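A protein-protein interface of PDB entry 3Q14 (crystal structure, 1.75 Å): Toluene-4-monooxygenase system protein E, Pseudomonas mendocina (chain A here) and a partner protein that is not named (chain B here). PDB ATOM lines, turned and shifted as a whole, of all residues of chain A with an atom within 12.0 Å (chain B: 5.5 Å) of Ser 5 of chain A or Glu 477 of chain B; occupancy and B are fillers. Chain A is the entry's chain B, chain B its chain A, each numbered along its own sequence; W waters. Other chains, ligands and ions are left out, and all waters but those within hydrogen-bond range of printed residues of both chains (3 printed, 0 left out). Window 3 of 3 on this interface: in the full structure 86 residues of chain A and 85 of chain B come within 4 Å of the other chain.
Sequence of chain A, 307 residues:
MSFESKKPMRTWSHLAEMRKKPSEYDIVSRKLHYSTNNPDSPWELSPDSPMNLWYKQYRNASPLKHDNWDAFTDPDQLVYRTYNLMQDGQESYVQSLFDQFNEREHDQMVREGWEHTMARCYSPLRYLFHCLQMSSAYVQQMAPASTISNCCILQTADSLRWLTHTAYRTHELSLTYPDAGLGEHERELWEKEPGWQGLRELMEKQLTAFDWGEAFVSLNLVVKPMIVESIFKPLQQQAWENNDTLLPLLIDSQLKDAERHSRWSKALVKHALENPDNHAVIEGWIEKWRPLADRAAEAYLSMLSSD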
ATOM      1  N   SER A   2      -7.676   6.264  26.129  1.00  0.00           N
ATOM      2  CA  SER A   2      -7.548   5.923  24.716  1.00  0.00           C
ATOM      3  C   SER A   2      -6.334   6.615  24.090  1.00  0.00           C
ATOM      4  O   SER A   2      -5.950   7.711  24.504  1.00  0.00           O
ATOM      5  CB  SER A   2      -8.829   6.300  23.963  1.00  0.00           C
ATOM      6  OG  SER A   2      -8.827   5.783  22.643  1.00  0.00           O
ATOM      7  N   PHE A   3      -5.724   5.968  23.101  1.00  0.00           N
ATOM      8  CA  PHE A   3      -4.606   6.569  22.378  1.00  0.00           C
ATOM      9  C   PHE A   3      -5.124   7.562  21.343  1.00  0.00           C
ATOM     10  O   PHE A   3      -6.287   7.512  20.944  1.00  0.00           O
ATOM     11  CB  PHE A   3      -3.758   5.501  21.681  1.00  0.00           C
ATOM     12  CG  PHE A   3      -2.872   4.726  22.610  1.00  0.00           C
ATOM     13  CD1 PHE A   3      -1.640   5.233  22.995  1.00  0.00           C
ATOM     14  CD2 PHE A   3      -3.267   3.491  23.097  1.00  0.00           C
ATOM     15  CE1 PHE A   3      -0.819   4.523  23.854  1.00  0.00           C
ATOM     16  CE2 PHE A   3      -2.450   2.775  23.955  1.00  0.00           C
ATOM     17  CZ  PHE A   3      -1.224   3.291  24.334  1.00  0.00           C
ATOM     18  N   GLU A   4      -4.258   8.469  20.912  1.00  0.00           N
ATOM     19  CA  GLU A   4      -4.620   9.391  19.843  1.00  0.00           C
ATOM     20  C   GLU A   4      -3.846   9.062  18.582  1.00  0.00           C
ATOM     21  O   GLU A   4      -2.761   8.484  18.637  1.00  0.00           O
ATOM     22  CB  GLU A   4      -4.378  10.839  20.269  1.00  0.00           C
ATOM     23  CG  GLU A   4      -3.106  11.044  21.067  1.00  0.00           C
ATOM     24  CD  GLU A   4      -3.130  12.323  21.884  1.00  0.00           C
ATOM     25  OE1 GLU A   4      -4.098  13.105  21.741  1.00  0.00           O
ATOM     26  OE2 GLU A   4      -2.183  12.541  22.673  1.00  0.00           O
ATOM     27  N   SER A   5      -4.414   9.415  17.438  1.00  0.00           N
ATOM     28  CA  SER A   5      -3.725   9.200  16.181  1.00  0.00           C
ATOM     29  C   SER A   5      -2.939  10.459  15.858  1.00  0.00           C
ATOM     30  O   SER A   5      -3.462  11.571  15.919  1.00  0.00           O
ATOM     31  CB  SER A   5      -4.720   8.866  15.071  1.00  0.00           C
ATOM     32  OG  SER A   5      -4.044   8.415  13.911  1.00  0.00           O
ATOM     33  N   LYS A   6      -1.667  10.280  15.540  1.00  0.00           N
ATOM     34  CA  LYS A   6      -0.806  11.397  15.237  1.00  0.00           C
ATOM     35  C   LYS A   6      -0.140  11.105  13.907  1.00  0.00           C
ATOM     36  O   LYS A   6      -0.053   9.954  13.487  1.00  0.00           O
ATOM     37  CB  LYS A   6       0.245  11.579  16.332  1.00  0.00           C
ATOM     38  CG  LYS A   6      -0.331  11.821  17.733  1.00  0.00           C
ATOM     39  CD  LYS A   6       0.736  12.407  18.644  1.00  0.00           C
ATOM     40  CE  LYS A   6       0.163  12.869  19.971  1.00  0.00           C
ATOM     41  NZ  LYS A   6      -0.050  11.735  20.899  1.00  0.00           N
ATOM     42  N   LYS A   7       0.296  12.147  13.228  1.00  0.00           N
ATOM     43  CA  LYS A   7       0.965  11.944  11.960  1.00  0.00           C
ATOM     44  C   LYS A   7       2.465  11.976  12.177  1.00  0.00           C
ATOM     45  O   LYS A   7       2.929  12.396  13.239  1.00  0.00           O
ATOM     46  CB  LYS A   7       0.539  13.006  10.957  1.00  0.00           C
ATOM     47  CG  LYS A   7       0.568  14.411  11.497  1.00  0.00           C
ATOM     48  CD  LYS A   7      -0.574  15.219  10.892  1.00  0.00           C
ATOM     49  CE  LYS A   7      -0.447  16.695  11.222  1.00  0.00           C
ATOM     50  NZ  LYS A   7       0.813  17.264  10.660  1.00  0.00           N
ATOM     51  N   PRO A   8       3.225  11.513  11.176  1.00  0.00           N
ATOM     52  CA  PRO A   8       4.687  11.572  11.233  1.00  0.00           C
ATOM     53  C   PRO A   8       5.192  12.981  11.531  1.00  0.00           C
ATOM     54  O   PRO A   8       4.600  13.972  11.084  1.00  0.00           O
ATOM     55  CB  PRO A   8       5.094  11.158   9.818  1.00  0.00           C
ATOM     56  CG  PRO A   8       4.019  10.223   9.395  1.00  0.00           C
ATOM     57  CD  PRO A   8       2.753  10.821   9.963  1.00  0.00           C
ATOM     58  N   MET A   9       6.283  13.057  12.284  1.00  0.00           N
ATOM     59  CA  MET A   9       6.907  14.323  12.630  1.00  0.00           C
ATOM     60  C   MET A   9       8.084  14.535  11.690  1.00  0.00           C
ATOM     61  O   MET A   9       8.634  13.568  11.159  1.00  0.00           O
ATOM     62  CB  MET A   9       7.351  14.309  14.092  1.00  0.00           C
ATOM     63  CG  MET A   9       6.180  14.203  15.085  1.00  0.00           C
ATOM     64  SD  MET A   9       6.686  13.785  16.768  1.00  0.00           S
ATOM     65  CE  MET A   9       7.233  12.085  16.566  1.00  0.00           C
ATOM     66  N   ASP B 152       7.301   7.714   8.900  1.00  0.00           N
ATOM     67  CA  ASP B 152       6.809   6.671   9.786  1.00  0.00           C
ATOM     68  C   ASP B 152       7.212   6.968  11.231  1.00  0.00           C
ATOM     69  O   ASP B 152       8.400   7.044  11.540  1.00  0.00           O
ATOM     70  CB  ASP B 152       7.420   5.337   9.335  1.00  0.00           C
ATOM     71  CG  ASP B 152       6.750   4.132   9.969  1.00  0.00           C
ATOM     72  OD1 ASP B 152       6.463   4.158  11.186  1.00  0.00           O
ATOM     73  OD2 ASP B 152       6.507   3.151   9.235  1.00  0.00           O
ATOM     74  N   ARG B 153       6.223   7.125  12.111  1.00  0.00           N
ATOM     75  CA  ARG B 153       6.499   7.456  13.506  1.00  0.00           C
ATOM     76  C   ARG B 153       7.346   6.385  14.210  1.00  0.00           C
ATOM     77  O   ARG B 153       8.020   6.672  15.200  1.00  0.00           O
ATOM     78  CB  ARG B 153       5.194   7.710  14.283  1.00  0.00           C
ATOM     79  CG  ARG B 153       4.446   8.974  13.855  1.00  0.00           C
ATOM     80  CD  ARG B 153       3.235   9.217  14.760  1.00  0.00           C
ATOM     81  NE  ARG B 153       3.638   9.430  16.147  1.00  0.00           N
ATOM     82  CZ  ARG B 153       3.833  10.624  16.699  1.00  0.00           C
ATOM     83  NH1 ARG B 153       3.654  11.731  15.989  1.00  0.00           N
ATOM     84  NH2 ARG B 153       4.201  10.715  17.970  1.00  0.00           N
ATOM     85  N   GLN B 154       7.339   5.156  13.707  1.00  0.00           N
ATOM     86  CA  GLN B 154       8.151   4.122  14.351  1.00  0.00           C
ATOM     87  C   GLN B 154       9.651   4.440  14.258  1.00  0.00           C
ATOM     88  O   GLN B 154      10.440   3.978  15.075  1.00  0.00           O
ATOM     89  CB  GLN B 154       7.845   2.728  13.798  1.00  0.00           C
ATOM     90  CG  GLN B 154       6.542   2.137  14.322  1.00  0.00           C
ATOM     91  CD  GLN B 154       6.214   0.784  13.721  1.00  0.00           C
ATOM     92  OE1 GLN B 154       6.667   0.450  12.631  1.00  0.00           O
ATOM     93  NE2 GLN B 154       5.417  -0.009  14.440  1.00  0.00           N
ATOM     94  N   SER B 475       1.251   7.187  20.187  1.00  0.00           N
ATOM     95  CA  SER B 475       0.130   7.144  19.257  1.00  0.00           C
ATOM     96  C   SER B 475      -0.109   5.724  18.789  1.00  0.00           C
ATOM     97  O   SER B 475       0.738   4.854  18.945  1.00  0.00           O
ATOM     98  CB  SER B 475       0.371   8.057  18.053  1.00  0.00           C
ATOM     99  OG  SER B 475       1.004   7.359  16.992  1.00  0.00           O
ATOM    100  N   ILE B 476      -1.267   5.488  18.194  1.00  0.00           N
ATOM    101  CA  ILE B 476      -1.609   4.133  17.771  1.00  0.00           C
ATOM    102  C   ILE B 476      -0.717   3.603  16.634  1.00  0.00           C
ATOM    103  O   ILE B 476      -0.421   2.411  16.582  1.00  0.00           O
ATOM    104  CB  ILE B 476      -3.119   4.002  17.445  1.00  0.00           C
ATOM    105  CG1 ILE B 476      -3.425   2.647  16.799  1.00  0.00           C
ATOM    106  CG2 ILE B 476      -3.580   5.161  16.579  1.00  0.00           C
ATOM    107  CD1 ILE B 476      -3.588   2.701  15.294  1.00  0.00           C
ATOM    108  N   GLU B 477      -0.272   4.485  15.739  1.00  0.00           N
ATOM    109  CA  GLU B 477       0.560   4.065  14.607  1.00  0.00           C
ATOM    110  C   GLU B 477       1.904   3.484  15.018  1.00  0.00           C
ATOM    111  O   GLU B 477       2.554   2.785  14.230  1.00  0.00           O
ATOM    112  CB  GLU B 477       0.821   5.227  13.652  1.00  0.00           C
ATOM    113  CG  GLU B 477      -0.409   5.737  12.930  1.00  0.00           C
ATOM    114  CD  GLU B 477      -1.288   6.593  13.819  1.00  0.00           C
ATOM    115  OE1 GLU B 477      -0.738   7.408  14.595  1.00  0.00           O
ATOM    116  OE2 GLU B 477      -2.526   6.446  13.740  1.00  0.00           O
ATOM    117  N   GLU B 478       2.336   3.787  16.237  1.00  0.00           N
ATOM    118  CA  GLU B 478       3.676   3.395  16.679  1.00  0.00           C
ATOM    119  C   GLU B 478       3.743   1.942  17.122  1.00  0.00           C
ATOM    120  O   GLU B 478       4.805   1.315  17.078  1.00  0.00           O
ATOM    121  CB  GLU B 478       4.142   4.308  17.811  1.00  0.00           C
ATOM    122  CG  GLU B 478       4.205   5.767  17.424  1.00  0.00           C
ATOM    123  CD  GLU B 478       4.561   6.658  18.590  1.00  0.00           C
ATOM    124  OE1 GLU B 478       4.725   6.125  19.703  1.00  0.00           O
ATOM    125  OE2 GLU B 478       4.670   7.888  18.393  1.00  0.00           O
ATOM    126  N   MET B 479       2.606   1.408  17.556  1.00  0.00           N
ATOM    127  CA  MET B 479       2.562   0.042  18.060  1.00  0.00           C
ATOM    128  C   MET B 479       2.720  -0.955  16.919  1.00  0.00           C
ATOM    129  O   MET B 479       2.232  -0.724  15.814  1.00  0.00           O
ATOM    130  CB  MET B 479       1.258  -0.180  18.833  1.00  0.00           C
ATOM    131  CG  MET B 479       1.161   0.711  20.070  1.00  0.00           C
ATOM    132  SD  MET B 479      -0.526   1.035  20.624  1.00  0.00           S
ATOM    133  CE  MET B 479      -1.383  -0.323  19.834  1.00  0.00           C
HETATM  134  O   HOH W   1       2.304  14.633  14.909  1.00  0.00           O
HETATM  135  O   HOH W   2       3.400  14.666  17.487  1.00  0.00           O
HETATM  136  O   HOH W   3       4.656  13.180  19.724  1.00  0.00           O
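Phe 3 of chain A touches none of the printed residues of chain B.
Of the printed residues of chain B, Lys 6 of chain A touches Arg 153, Ser 475 and Glu 477.
Of the printed residues of chain B, Lys 7 of chain A touches Arg 153 (2.9 Å).
Of the printed residues of chain B, Met 9 of chain A touches Arg 153 (3.6 Å).
Arg 153 of chain B touches just these residues of chain A: Lys 6 (3.4 Å), Lys 7 (2.9 Å), Pro 8 (3.7 Å) and Met 9 (3.6 Å).
Ile 476 of chain B touches one residue of chain A.
Of chain A, only Ser 5 (2.5 Å) and Lys 6 (2.9 Å) come within 4 Å of Glu 477 of chain B.
No residue of chain A comes within 4 Å of Met 479 of chain B.
The nearest residue of chain B that does not touch Ser 5 of chain A is Ile 476 of chain B (4.1 Å).
Of the 8 printed residues of chain B, 4 touch a printed residue of chain A.
Hydrophobic or aromatic side chains of chain B that line the printed part of chain A: Ile 476.
Hydrophobic or aromatic side chains of chain A that line the printed part of chain B: Met 9.
The guanidinium group (NE) of Arg 153 of chain B is in hydrogen-bond range of the side-chain hydroxyl (OG) of Ser 475 of chain B (3.5 Å).
The guanidinium group (NH2) of Arg 153 of chain B lies within salt-bridge range of the side-chain carboxylate (OE2) of Glu 478 of chain B.
The side-chain hydroxyl of Ser 475 of chain B sits at hydrogen-bond distance from the side-chain carboxylate of Glu 477 of chain B (3.0 Å).
The side-chain carboxylate of Glu 4 of chain A lies within salt-bridge range of the side-chain amino group of Lys 6 of chain A, at 2.9 Å.
CB of Ser 475 of chain B touches O of Glu 4 of chain A, 3.2 Å away.
Lys 6 of chain A touches Arg 153 of chain B (CB to NH1, 3.4 Å).
Lys 6 of chain A touches Ser 475 of chain B (CG to CB, 3.8 Å).
CG of Arg 153 of chain B touches CA of Pro 8 of chain A, at 3.7 Å.
The guanidinium group (NH1) of Arg 153 of chain B sits at hydrogen-bond distance from the backbone carbonyl oxygen (O) of Lys 7 of chain A, at 2.9 Å.
The guanidinium group (NH1) of Arg 153 of chain B lies close to the side-chain sulfur (SD) of Met 9 of chain A (3.7 Å).
The backbone carbonyl oxygen (O) of Glu 4 of chain A sits at hydrogen-bond distance from the backbone NH (N) of Ile 476 of chain B, at 3.4 Å.
OG of Ser 5 of chain A is in hydrogen-bond range of OE2 of Glu 477 of chain B (2.5 Å).
N of Lys 6 of chain A sits at hydrogen-bond distance from OE1 of Glu 477 of chain B (3.2 Å).
Water W1 bridges O of Lys 7 of chain A (2.9 Å) and NH1 of Arg 153 of chain B (3.4 Å).
Water W3 bridges NH2 of Arg 153 of chain B (3.1 Å) and SD of Met 9 of chain A (3.6 Å).
Water W2 lies within hydrogen-bond range of NH1 of Arg 153 of chain B and SD of Met 9 of chain A.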
